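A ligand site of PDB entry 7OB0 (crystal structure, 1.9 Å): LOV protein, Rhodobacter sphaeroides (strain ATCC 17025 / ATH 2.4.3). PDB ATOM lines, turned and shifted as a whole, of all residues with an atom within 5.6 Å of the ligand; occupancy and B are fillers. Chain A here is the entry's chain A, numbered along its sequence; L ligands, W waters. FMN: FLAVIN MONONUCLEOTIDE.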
ATOM      1  N   THR A  21      32.011  -5.747 -21.618  1.00  0.00           N
ATOM      2  CA  THR A  21      31.306  -5.757 -20.347  1.00  0.00           C
ATOM      3  C   THR A  21      31.334  -7.176 -19.795  1.00  0.00           C
ATOM      4  O   THR A  21      31.421  -8.138 -20.557  1.00  0.00           O
ATOM      5  CB  THR A  21      29.844  -5.308 -20.499  1.00  0.00           C
ATOM      6  OG1 THR A  21      29.238  -6.063 -21.548  1.00  0.00           O
ATOM      7  CG2 THR A  21      29.770  -3.814 -20.852  1.00  0.00           C
ATOM      8  N   LEU A  22      31.236  -7.298 -18.471  1.00  0.00           N
ATOM      9  CA  LEU A  22      31.186  -8.611 -17.832  1.00  0.00           C
ATOM     10  C   LEU A  22      30.051  -8.605 -16.832  1.00  0.00           C
ATOM     11  O   LEU A  22      29.933  -7.659 -16.047  1.00  0.00           O
ATOM     12  CB  LEU A  22      32.515  -8.982 -17.160  1.00  0.00           C
ATOM     13  CG  LEU A  22      32.717 -10.468 -16.863  1.00  0.00           C
ATOM     14  CD1 LEU A  22      33.021 -11.230 -18.163  1.00  0.00           C
ATOM     15  CD2 LEU A  22      33.868 -10.637 -15.895  1.00  0.00           C
ATOM     16  N   VAL A  23      29.213  -9.635 -16.856  1.00  0.00           N
ATOM     17  CA  VAL A  23      28.033  -9.735 -16.031  1.00  0.00           C
ATOM     18  C   VAL A  23      28.177 -10.952 -15.130  1.00  0.00           C
ATOM     19  O   VAL A  23      28.544 -12.028 -15.608  1.00  0.00           O
ATOM     20  CB  VAL A  23      26.760  -9.824 -16.886  1.00  0.00           C
ATOM     21  CG1 VAL A  23      25.607 -10.356 -16.096  1.00  0.00           C
ATOM     22  CG2 VAL A  23      26.407  -8.423 -17.468  1.00  0.00           C
ATOM     23  N   MET A  25      26.945 -13.998 -13.322  1.00  0.00           N
ATOM     24  CA  MET A  25      25.852 -14.929 -13.558  1.00  0.00           C
ATOM     25  C   MET A  25      25.405 -15.637 -12.275  1.00  0.00           C
ATOM     26  O   MET A  25      24.447 -16.429 -12.309  1.00  0.00           O
ATOM     27  CB  MET A  25      26.303 -15.965 -14.595  1.00  0.00           C
ATOM     28  CG  MET A  25      26.168 -15.569 -16.078  1.00  0.00           C
ATOM     29  SD  MET A  25      24.870 -14.439 -16.581  1.00  0.00           S
ATOM     30  CE  MET A  25      23.759 -15.667 -17.260  1.00  0.00           C
ATOM     31  N   GLN A  30      21.883 -10.515 -12.193  1.00  0.00           N
ATOM     32  CA  GLN A  30      22.868 -10.460 -13.268  1.00  0.00           C
ATOM     33  C   GLN A  30      23.515  -9.077 -13.380  1.00  0.00           C
ATOM     34  O   GLN A  30      23.430  -8.432 -14.437  1.00  0.00           O
ATOM     35  CB  GLN A  30      22.251 -10.893 -14.594  1.00  0.00           C
ATOM     36  CG  GLN A  30      22.116 -12.435 -14.679  1.00  0.00           C
ATOM     37  CD  GLN A  30      21.165 -12.920 -15.756  1.00  0.00           C
ATOM     38  OE1 GLN A  30      20.713 -12.157 -16.610  1.00  0.00           O
ATOM     39  NE2 GLN A  30      20.860 -14.213 -15.729  1.00  0.00           N
ATOM     40  N   PHE A  39      33.372   1.090 -23.646  1.00  0.00           N
ATOM     41  CA  PHE A  39      31.958   0.973 -23.305  1.00  0.00           C
ATOM     42  C   PHE A  39      31.468   2.231 -22.603  1.00  0.00           C
ATOM     43  O   PHE A  39      30.359   2.707 -22.885  1.00  0.00           O
ATOM     44  CB  PHE A  39      31.705  -0.252 -22.410  1.00  0.00           C
ATOM     45  CG  PHE A  39      30.247  -0.379 -21.993  1.00  0.00           C
ATOM     46  CD1 PHE A  39      29.336  -1.013 -22.832  1.00  0.00           C
ATOM     47  CD2 PHE A  39      29.804   0.136 -20.787  1.00  0.00           C
ATOM     48  CE1 PHE A  39      28.013  -1.117 -22.478  1.00  0.00           C
ATOM     49  CE2 PHE A  39      28.470   0.026 -20.426  1.00  0.00           C
ATOM     50  CZ  PHE A  39      27.574  -0.611 -21.273  1.00  0.00           C
ATOM     51  N   MET A  42      30.962   5.067 -25.099  1.00  0.00           N
ATOM     52  CA  MET A  42      29.796   4.888 -25.942  1.00  0.00           C
ATOM     53  C   MET A  42      28.513   5.221 -25.193  1.00  0.00           C
ATOM     54  O   MET A  42      27.600   5.820 -25.766  1.00  0.00           O
ATOM     55  CB  MET A  42      29.765   3.467 -26.504  1.00  0.00           C
ATOM     56  CG  MET A  42      28.461   3.085 -27.203  1.00  0.00           C
ATOM     57  SD  MET A  42      28.403   1.341 -27.626  1.00  0.00           S
ATOM     58  CE  MET A  42      27.931   0.707 -26.029  1.00  0.00           C
ATOM     59  N   ASN A  54      21.871  -4.314 -13.717  1.00  0.00           N
ATOM     60  CA  ASN A  54      21.685  -5.084 -14.939  1.00  0.00           C
ATOM     61  C   ASN A  54      21.822  -4.166 -16.146  1.00  0.00           C
ATOM     62  O   ASN A  54      21.407  -3.016 -16.111  1.00  0.00           O
ATOM     63  CB  ASN A  54      20.320  -5.767 -14.983  1.00  0.00           C
ATOM     64  CG  ASN A  54      20.164  -6.694 -16.176  1.00  0.00           C
ATOM     65  OD1 ASN A  54      19.948  -6.262 -17.319  1.00  0.00           O
ATOM     66  ND2 ASN A  54      20.295  -7.992 -15.926  1.00  0.00           N
ATOM     67  N   CYS A  55      22.374  -4.692 -17.229  1.00  0.00           N
ATOM     68  CA  CYS A  55      22.695  -3.882 -18.399  1.00  0.00           C
ATOM     69  C   CYS A  55      21.459  -3.319 -19.078  1.00  0.00           C
ATOM     70  O   CYS A  55      21.601  -2.488 -19.984  1.00  0.00           O
ATOM     71  CB  CYS A  55      23.497  -4.717 -19.391  1.00  0.00           C
ATOM     72  SG  CYS A  55      25.244  -4.826 -18.962  1.00  0.00           S
ATOM     73  N   ARG A  56      20.260  -3.771 -18.698  1.00  0.00           N
ATOM     74  CA  ARG A  56      19.044  -3.266 -19.316  1.00  0.00           C
ATOM     75  C   ARG A  56      18.778  -1.789 -19.003  1.00  0.00           C
ATOM     76  O   ARG A  56      17.802  -1.246 -19.533  1.00  0.00           O
ATOM     77  CB  ARG A  56      17.848  -4.115 -18.863  1.00  0.00           C
ATOM     78  CG  ARG A  56      17.293  -3.730 -17.503  1.00  0.00           C
ATOM     79  CD  ARG A  56      16.086  -4.589 -17.137  1.00  0.00           C
ATOM     80  NE  ARG A  56      16.335  -5.998 -17.384  1.00  0.00           N
ATOM     81  CZ  ARG A  56      16.786  -6.849 -16.478  1.00  0.00           C
ATOM     82  NH1 ARG A  56      17.016  -6.472 -15.229  1.00  0.00           N
ATOM     83  NH2 ARG A  56      17.013  -8.118 -16.820  1.00  0.00           N
ATOM     84  N   LEU A  58      20.255   0.456 -20.267  1.00  0.00           N
ATOM     85  CA  LEU A  58      20.456   1.077 -21.567  1.00  0.00           C
ATOM     86  C   LEU A  58      19.216   1.027 -22.440  1.00  0.00           C
ATOM     87  O   LEU A  58      19.227   1.609 -23.533  1.00  0.00           O
ATOM     88  CB  LEU A  58      21.616   0.395 -22.297  1.00  0.00           C
ATOM     89  CG  LEU A  58      22.981   0.580 -21.647  1.00  0.00           C
ATOM     90  CD1 LEU A  58      24.037  -0.283 -22.338  1.00  0.00           C
ATOM     91  CD2 LEU A  58      23.388   2.052 -21.703  1.00  0.00           C
ATOM     92  N   GLN A  59      18.164   0.331 -22.018  1.00  0.00           N
ATOM     93  CA  GLN A  59      16.948   0.163 -22.793  1.00  0.00           C
ATOM     94  C   GLN A  59      15.826   0.982 -22.181  1.00  0.00           C
ATOM     95  O   GLN A  59      15.966   1.537 -21.086  1.00  0.00           O
ATOM     96  CB  GLN A  59      16.533  -1.312 -22.852  1.00  0.00           C
ATOM     97  CG  GLN A  59      17.454  -2.170 -23.691  1.00  0.00           C
ATOM     98  CD  GLN A  59      17.084  -3.644 -23.600  1.00  0.00           C
ATOM     99  OE1 GLN A  59      15.957  -4.020 -23.887  1.00  0.00           O
ATOM    100  NE2 GLN A  59      18.024  -4.467 -23.180  1.00  0.00           N
ATOM    101  N   ASN A  64      12.682  -3.995 -27.987  1.00  0.00           N
ATOM    102  CA  ASN A  64      13.591  -5.131 -28.191  1.00  0.00           C
ATOM    103  C   ASN A  64      13.022  -6.450 -27.662  1.00  0.00           C
ATOM    104  O   ASN A  64      13.779  -7.318 -27.222  1.00  0.00           O
ATOM    105  CB  ASN A  64      14.947  -4.877 -27.514  1.00  0.00           C
ATOM    106  CG  ASN A  64      15.505  -3.506 -27.815  1.00  0.00           C
ATOM    107  OD1 ASN A  64      15.813  -3.199 -28.958  1.00  0.00           O
ATOM    108  ND2 ASN A  64      15.629  -2.672 -26.781  1.00  0.00           N
ATOM    109  N   ALA A  67      14.470  -9.645 -29.224  1.00  0.00           N
ATOM    110  CA  ALA A  67      15.880  -9.748 -28.862  1.00  0.00           C
ATOM    111  C   ALA A  67      16.053 -10.096 -27.385  1.00  0.00           C
ATOM    112  O   ALA A  67      16.930 -10.887 -27.036  1.00  0.00           O
ATOM    113  CB  ALA A  67      16.594  -8.430 -29.188  1.00  0.00           C
ATOM    114  N   ARG A  68      15.218  -9.514 -26.517  1.00  0.00           N
ATOM    115  CA  ARG A  68      15.329  -9.791 -25.082  1.00  0.00           C
ATOM    116  C   ARG A  68      14.970 -11.234 -24.776  1.00  0.00           C
ATOM    117  O   ARG A  68      15.633 -11.885 -23.944  1.00  0.00           O
ATOM    118  CB  ARG A  68      14.443  -8.834 -24.277  1.00  0.00           C
ATOM    119  CG  ARG A  68      14.962  -7.403 -24.165  1.00  0.00           C
ATOM    120  CD  ARG A  68      13.841  -6.413 -23.823  1.00  0.00           C
ATOM    121  NE  ARG A  68      12.928  -6.973 -22.827  1.00  0.00           N
ATOM    122  CZ  ARG A  68      11.620  -6.731 -22.763  1.00  0.00           C
ATOM    123  NH1 ARG A  68      11.031  -5.895 -23.605  1.00  0.00           N
ATOM    124  NH2 ARG A  68      10.895  -7.324 -21.825  1.00  0.00           N
ATOM    125  N   ALA A  69      13.940 -11.767 -25.418  1.00  0.00           N
ATOM    126  CA  ALA A  69      13.604 -13.178 -25.236  1.00  0.00           C
ATOM    127  C   ALA A  69      14.755 -14.068 -25.696  1.00  0.00           C
ATOM    128  O   ALA A  69      15.070 -15.061 -25.034  1.00  0.00           O
ATOM    129  CB  ALA A  69      12.318 -13.521 -25.987  1.00  0.00           C
ATOM    130  N   ILE A  71      17.962 -13.256 -25.767  1.00  0.00           N
ATOM    131  CA  ILE A  71      19.034 -13.096 -24.794  1.00  0.00           C
ATOM    132  C   ILE A  71      18.770 -13.949 -23.565  1.00  0.00           C
ATOM    133  O   ILE A  71      19.657 -14.662 -23.084  1.00  0.00           O
ATOM    134  CB  ILE A  71      19.208 -11.616 -24.409  1.00  0.00           C
ATOM    135  CG1 ILE A  71      19.783 -10.791 -25.568  1.00  0.00           C
ATOM    136  CG2 ILE A  71      20.131 -11.474 -23.199  1.00  0.00           C
ATOM    137  CD1 ILE A  71      19.751  -9.275 -25.302  1.00  0.00           C
ATOM    138  N   ARG A  72      17.549 -13.869 -23.033  1.00  0.00           N
ATOM    139  CA  ARG A  72      17.230 -14.638 -21.843  1.00  0.00           C
ATOM    140  C   ARG A  72      17.443 -16.129 -22.083  1.00  0.00           C
ATOM    141  O   ARG A  72      17.996 -16.820 -21.221  1.00  0.00           O
ATOM    142  CB  ARG A  72      15.793 -14.347 -21.389  1.00  0.00           C
ATOM    143  CG  ARG A  72      15.642 -12.935 -20.820  1.00  0.00           C
ATOM    144  CD  ARG A  72      14.300 -12.721 -20.095  1.00  0.00           C
ATOM    145  NE  ARG A  72      14.275 -13.329 -18.772  1.00  0.00           N
ATOM    146  CZ  ARG A  72      14.845 -12.815 -17.690  1.00  0.00           C
ATOM    147  NH1 ARG A  72      15.525 -11.671 -17.741  1.00  0.00           N
ATOM    148  NH2 ARG A  72      14.758 -13.460 -16.538  1.00  0.00           N
ATOM    149  N   LEU A  75      21.297 -16.765 -22.201  1.00  0.00           N
ATOM    150  CA  LEU A  75      21.889 -16.704 -20.871  1.00  0.00           C
ATOM    151  C   LEU A  75      21.546 -17.941 -20.050  1.00  0.00           C
ATOM    152  O   LEU A  75      22.412 -18.521 -19.386  1.00  0.00           O
ATOM    153  CB  LEU A  75      21.425 -15.440 -20.144  1.00  0.00           C
ATOM    154  CG  LEU A  75      21.794 -14.103 -20.793  1.00  0.00           C
ATOM    155  CD1 LEU A  75      21.323 -12.937 -19.904  1.00  0.00           C
ATOM    156  CD2 LEU A  75      23.278 -14.019 -21.041  1.00  0.00           C
ATOM    157  N   LEU A  85      20.120  -4.210 -30.538  1.00  0.00           N
ATOM    158  CA  LEU A  85      19.247  -3.589 -29.552  1.00  0.00           C
ATOM    159  C   LEU A  85      19.197  -2.089 -29.766  1.00  0.00           C
ATOM    160  O   LEU A  85      20.207  -1.467 -30.118  1.00  0.00           O
ATOM    161  CB  LEU A  85      19.759  -3.851 -28.140  1.00  0.00           C
ATOM    162  CG  LEU A  85      19.895  -5.326 -27.755  1.00  0.00           C
ATOM    163  CD1 LEU A  85      20.631  -5.465 -26.445  1.00  0.00           C
ATOM    164  CD2 LEU A  85      18.512  -5.924 -27.647  1.00  0.00           C
ATOM    165  N   ARG A  86      18.015  -1.505 -29.557  1.00  0.00           N
ATOM    166  CA  ARG A  86      17.917  -0.054 -29.437  1.00  0.00           C
ATOM    167  C   ARG A  86      18.291   0.338 -28.013  1.00  0.00           C
ATOM    168  O   ARG A  86      17.653  -0.124 -27.056  1.00  0.00           O
ATOM    169  CB  ARG A  86      16.506   0.400 -29.800  1.00  0.00           C
ATOM    170  CG  ARG A  86      16.207   1.840 -29.416  1.00  0.00           C
ATOM    171  CD  ARG A  86      16.938   2.833 -30.311  1.00  0.00           C
ATOM    172  NE  ARG A  86      16.999   2.395 -31.708  1.00  0.00           N
ATOM    173  CZ  ARG A  86      16.210   2.843 -32.673  1.00  0.00           C
ATOM    174  NH1 ARG A  86      15.271   3.754 -32.443  1.00  0.00           N
ATOM    175  NH2 ARG A  86      16.362   2.369 -33.913  1.00  0.00           N
ATOM    176  N   ASN A  87      19.327   1.153 -27.872  1.00  0.00           N
ATOM    177  CA  ASN A  87      19.818   1.617 -26.573  1.00  0.00           C
ATOM    178  C   ASN A  87      19.788   3.152 -26.519  1.00  0.00           C
ATOM    179  O   ASN A  87      19.493   3.828 -27.501  1.00  0.00           O
ATOM    180  CB  ASN A  87      21.250   1.103 -26.315  1.00  0.00           C
ATOM    181  CG  ASN A  87      21.297  -0.345 -25.800  1.00  0.00           C
ATOM    182  OD1 ASN A  87      22.376  -0.871 -25.543  1.00  0.00           O
ATOM    183  ND2 ASN A  87      20.140  -0.952 -25.616  1.00  0.00           N
ATOM    184  N   ASN A  97      22.729  -0.940 -31.282  1.00  0.00           N
ATOM    185  CA  ASN A  97      23.856  -1.594 -30.646  1.00  0.00           C
ATOM    186  C   ASN A  97      23.835  -3.043 -31.099  1.00  0.00           C
ATOM    187  O   ASN A  97      22.883  -3.762 -30.805  1.00  0.00           O
ATOM    188  CB  ASN A  97      23.704  -1.447 -29.122  1.00  0.00           C
ATOM    189  CG  ASN A  97      24.694  -2.288 -28.318  1.00  0.00           C
ATOM    190  OD1 ASN A  97      25.523  -3.033 -28.852  1.00  0.00           O
ATOM    191  ND2 ASN A  97      24.615  -2.138 -27.001  1.00  0.00           N
ATOM    192  N   LEU A  99      25.055  -6.331 -30.250  1.00  0.00           N
ATOM    193  CA  LEU A  99      25.602  -6.905 -29.031  1.00  0.00           C
ATOM    194  C   LEU A  99      26.045  -8.347 -29.264  1.00  0.00           C
ATOM    195  O   LEU A  99      25.264  -9.168 -29.750  1.00  0.00           O
ATOM    196  CB  LEU A  99      24.552  -6.841 -27.915  1.00  0.00           C
ATOM    197  CG  LEU A  99      24.874  -7.591 -26.597  1.00  0.00           C
ATOM    198  CD1 LEU A  99      25.901  -6.834 -25.810  1.00  0.00           C
ATOM    199  CD2 LEU A  99      23.597  -7.789 -25.754  1.00  0.00           C
ATOM    200  N   LEU A 101      27.306 -11.688 -27.214  1.00  0.00           N
ATOM    201  CA  LEU A 101      27.349 -12.281 -25.881  1.00  0.00           C
ATOM    202  C   LEU A 101      28.147 -13.578 -25.937  1.00  0.00           C
ATOM    203  O   LEU A 101      28.002 -14.371 -26.882  1.00  0.00           O
ATOM    204  CB  LEU A 101      25.942 -12.571 -25.362  1.00  0.00           C
ATOM    205  CG  LEU A 101      25.128 -11.322 -25.029  1.00  0.00           C
ATOM    206  CD1 LEU A 101      23.672 -11.693 -24.711  1.00  0.00           C
ATOM    207  CD2 LEU A 101      25.766 -10.545 -23.909  1.00  0.00           C
ATOM    208  N   PHE A 114      28.952 -13.743 -18.047  1.00  0.00           N
ATOM    209  CA  PHE A 114      28.749 -13.516 -19.473  1.00  0.00           C
ATOM    210  C   PHE A 114      29.511 -12.282 -19.886  1.00  0.00           C
ATOM    211  O   PHE A 114      29.513 -11.275 -19.166  1.00  0.00           O
ATOM    212  CB  PHE A 114      27.272 -13.371 -19.853  1.00  0.00           C
ATOM    213  CG  PHE A 114      26.749 -14.511 -20.652  1.00  0.00           C
ATOM    214  CD1 PHE A 114      26.240 -15.638 -20.021  1.00  0.00           C
ATOM    215  CD2 PHE A 114      26.823 -14.497 -22.034  1.00  0.00           C
ATOM    216  CE1 PHE A 114      25.755 -16.708 -20.758  1.00  0.00           C
ATOM    217  CE2 PHE A 114      26.352 -15.571 -22.781  1.00  0.00           C
ATOM    218  CZ  PHE A 114      25.815 -16.691 -22.131  1.00  0.00           C
ATOM    219  N   LEU A 115      30.197 -12.382 -21.019  1.00  0.00           N
ATOM    220  CA  LEU A 115      30.885 -11.251 -21.630  1.00  0.00           C
ATOM    221  C   LEU A 115      29.967 -10.622 -22.671  1.00  0.00           C
ATOM    222  O   LEU A 115      29.295 -11.327 -23.427  1.00  0.00           O
ATOM    223  CB  LEU A 115      32.200 -11.701 -22.268  1.00  0.00           C
ATOM    224  CG  LEU A 115      32.996 -10.608 -22.968  1.00  0.00           C
ATOM    225  CD1 LEU A 115      34.484 -10.945 -22.889  1.00  0.00           C
ATOM    226  CD2 LEU A 115      32.571 -10.431 -24.441  1.00  0.00           C
ATOM    227  N   GLY A 116      29.928  -9.303 -22.709  1.00  0.00           N
ATOM    228  CA  GLY A 116      29.229  -8.582 -23.767  1.00  0.00           C
ATOM    229  C   GLY A 116      30.161  -7.619 -24.471  1.00  0.00           C
ATOM    230  O   GLY A 116      31.011  -7.004 -23.840  1.00  0.00           O
ATOM    231  N   GLN A 118      29.874  -4.491 -27.525  1.00  0.00           N
ATOM    232  CA  GLN A 118      28.880  -3.637 -28.171  1.00  0.00           C
ATOM    233  C   GLN A 118      29.510  -2.916 -29.358  1.00  0.00           C
ATOM    234  O   GLN A 118      30.474  -2.158 -29.188  1.00  0.00           O
ATOM    235  CB  GLN A 118      28.337  -2.635 -27.153  1.00  0.00           C
ATOM    236  CG  GLN A 118      27.609  -3.278 -25.948  1.00  0.00           C
ATOM    237  CD  GLN A 118      28.539  -3.774 -24.833  1.00  0.00           C
ATOM    238  OE1 GLN A 118      29.745  -3.542 -24.840  1.00  0.00           O
ATOM    239  NE2 GLN A 118      27.960  -4.507 -23.881  1.00  0.00           N
HETATM  240  N1  FMN L   1      21.387  -5.002 -23.092  1.00  0.00           N
HETATM  241  C2  FMN L   1      21.427  -3.782 -23.723  1.00  0.00           C
HETATM  242  O2  FMN L   1      20.360  -3.245 -24.007  1.00  0.00           O
HETATM  243  N3  FMN L   1      22.623  -3.177 -24.047  1.00  0.00           N
HETATM  244  C4  FMN L   1      23.809  -3.792 -23.727  1.00  0.00           C
HETATM  245  O4  FMN L   1      24.876  -3.269 -24.012  1.00  0.00           O
HETATM  246  C4A FMN L   1      23.780  -5.022 -23.076  1.00  0.00           C
HETATM  247  N5  FMN L   1      24.943  -5.653 -22.720  1.00  0.00           N
HETATM  248  C5A FMN L   1      24.870  -6.879 -22.073  1.00  0.00           C
HETATM  249  C6  FMN L   1      26.056  -7.510 -21.725  1.00  0.00           C
HETATM  250  C7  FMN L   1      26.014  -8.734 -21.075  1.00  0.00           C
HETATM  251  C7M FMN L   1      27.320  -9.393 -20.730  1.00  0.00           C
HETATM  252  C8  FMN L   1      24.802  -9.342 -20.774  1.00  0.00           C
HETATM  253  C8M FMN L   1      24.776 -10.670 -20.063  1.00  0.00           C
HETATM  254  C9  FMN L   1      23.606  -8.716 -21.114  1.00  0.00           C
HETATM  255  C9A FMN L   1      23.645  -7.481 -21.773  1.00  0.00           C
HETATM  256  N10 FMN L   1      22.488  -6.818 -22.110  1.00  0.00           N
HETATM  257  C10 FMN L   1      22.560  -5.612 -22.772  1.00  0.00           C
HETATM  258  C1' FMN L   1      21.112  -7.377 -21.899  1.00  0.00           C
HETATM  259  C2' FMN L   1      20.394  -7.137 -20.591  1.00  0.00           C
HETATM  260  O2' FMN L   1      21.366  -7.168 -19.580  1.00  0.00           O
HETATM  261  C3' FMN L   1      19.330  -8.238 -20.492  1.00  0.00           C
HETATM  262  O3' FMN L   1      19.959  -9.511 -20.397  1.00  0.00           O
HETATM  263  C4' FMN L   1      18.408  -8.222 -21.727  1.00  0.00           C
HETATM  264  O4' FMN L   1      17.722  -6.987 -21.796  1.00  0.00           O
HETATM  265  C5' FMN L   1      17.357  -9.332 -21.731  1.00  0.00           C
HETATM  266  O5' FMN L   1      16.861  -9.463 -20.413  1.00  0.00           O
HETATM  267  P   FMN L   1      15.529  -8.668 -19.954  1.00  0.00           P
HETATM  268  O1P FMN L   1      15.146  -9.230 -18.610  1.00  0.00           O
HETATM  269  O2P FMN L   1      14.397  -8.948 -20.942  1.00  0.00           O
HETATM  270  O3P FMN L   1      15.793  -7.169 -19.886  1.00  0.00           O
HETATM  271  O   HOH W   1      21.655  -9.674 -17.972  1.00  0.00           O
HETATM  272  O   HOH W   2      23.237  -7.353 -17.234  1.00  0.00           O
HETATM  273  O   HOH W   3      14.714  -4.889 -21.192  1.00  0.00           O
HETATM  274  O   HOH W   4      18.597 -10.973 -18.669  1.00  0.00           O
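ND2 of Asn 64 sits at hydrogen-bond distance from OE1 of Gln 59. N of Arg 56 is in hydrogen-bond range of OD1 of Asn 54, at 2.9 Å. The backbone carbonyl oxygen of Phe 114 sits at hydrogen-bond distance from the backbone NH of Val 23. The backbone carbonyl oxygen (O) of Gly 116 sits at hydrogen-bond distance from the backbone NH (N) of Thr 21 (2.7 Å). The side-chain amide nitrogen (ND2) of Asn 54 is in hydrogen-bond range of the backbone carbonyl oxygen (O) of Gln 30 (3.5 Å). The side-chain amide nitrogen (ND2) of Asn 97 lies within hydrogen-bond range of the side-chain amide oxygen (OD1) of Asn 87 (3.0 Å). The backbone NH (N) of Leu 85 sits at hydrogen-bond distance from the backbone carbonyl oxygen (O) of Asn 97. The backbone carbonyl oxygen (O) of Leu 58 sits close to the side-chain amide nitrogen (ND2) of Asn 87 (3.4 Å).
Water W4 lies within hydrogen-bond range of an oxygen (O3') of the ligand (2.6 Å), the side-chain amide oxygen of Gln 30 (3.2 Å) and the guanidinium group of Arg 72 (3.3 Å). Water W3 lies within hydrogen-bond range of O3P of the ligand, OE1 of Gln 59 and NE of Arg 68. Water W1 lies within hydrogen-bond range of O3' of the ligand (3.0 Å), ND2 of Asn 54 (3.0 Å) and OE1 of Gln 30 (3.0 Å). Water W2 lies within hydrogen-bond range of N of Cys 55 (2.8 Å), O of Gln 30 (3.0 Å), O2' of the ligand (3.0 Å) and ND2 of Asn 54 (3.3 Å).
O2' of the ligand is in hydrogen-bond range of OD1 of Asn 54. An oxygen (O3P) of the ligand lies within salt-bridge range of the guanidinium group of Arg 56 (2.8 Å). The guanidinium group (NH1) of Arg 72 lies within salt-bridge range of an oxygen (O1P) of the ligand. NE of Arg 68 is in salt-bridge range of O2P of the ligand (3.1 Å). An oxygen (O4) of the ligand is in hydrogen-bond range of the side-chain amide nitrogen (ND2) of Asn 97. O4 of the ligand lies within hydrogen-bond range of NE2 of Gln 118 (3.3 Å). An oxygen (O2) of the ligand sits at hydrogen-bond distance from the side-chain amide nitrogen of Gln 59, at 2.8 Å. A nitrogen (N3) of the ligand lies within hydrogen-bond range of the side-chain amide oxygen (OD1) of Asn 87, 2.8 Å away.
Merely in contact with the ligand: Cys 55 (3.3 Å), Gly 116 (3.3 Å), Phe 114 (3.3 Å), Leu 85 (3.3 Å), Leu 101 (3.4 Å), Ile 71 (3.4 Å), Leu 99 (3.4 Å), Thr 21 (3.5 Å), Leu 115 (3.5 Å), Val 23 (3.5 Å), Leu 58 (3.5 Å) and Leu 75 (3.7 Å). Hydrophobic or aromatic side chains that line the ligand: Val 23, Leu 58, Ile 71, Leu 75, Leu 85, Leu 99, Leu 101 and Phe 114.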
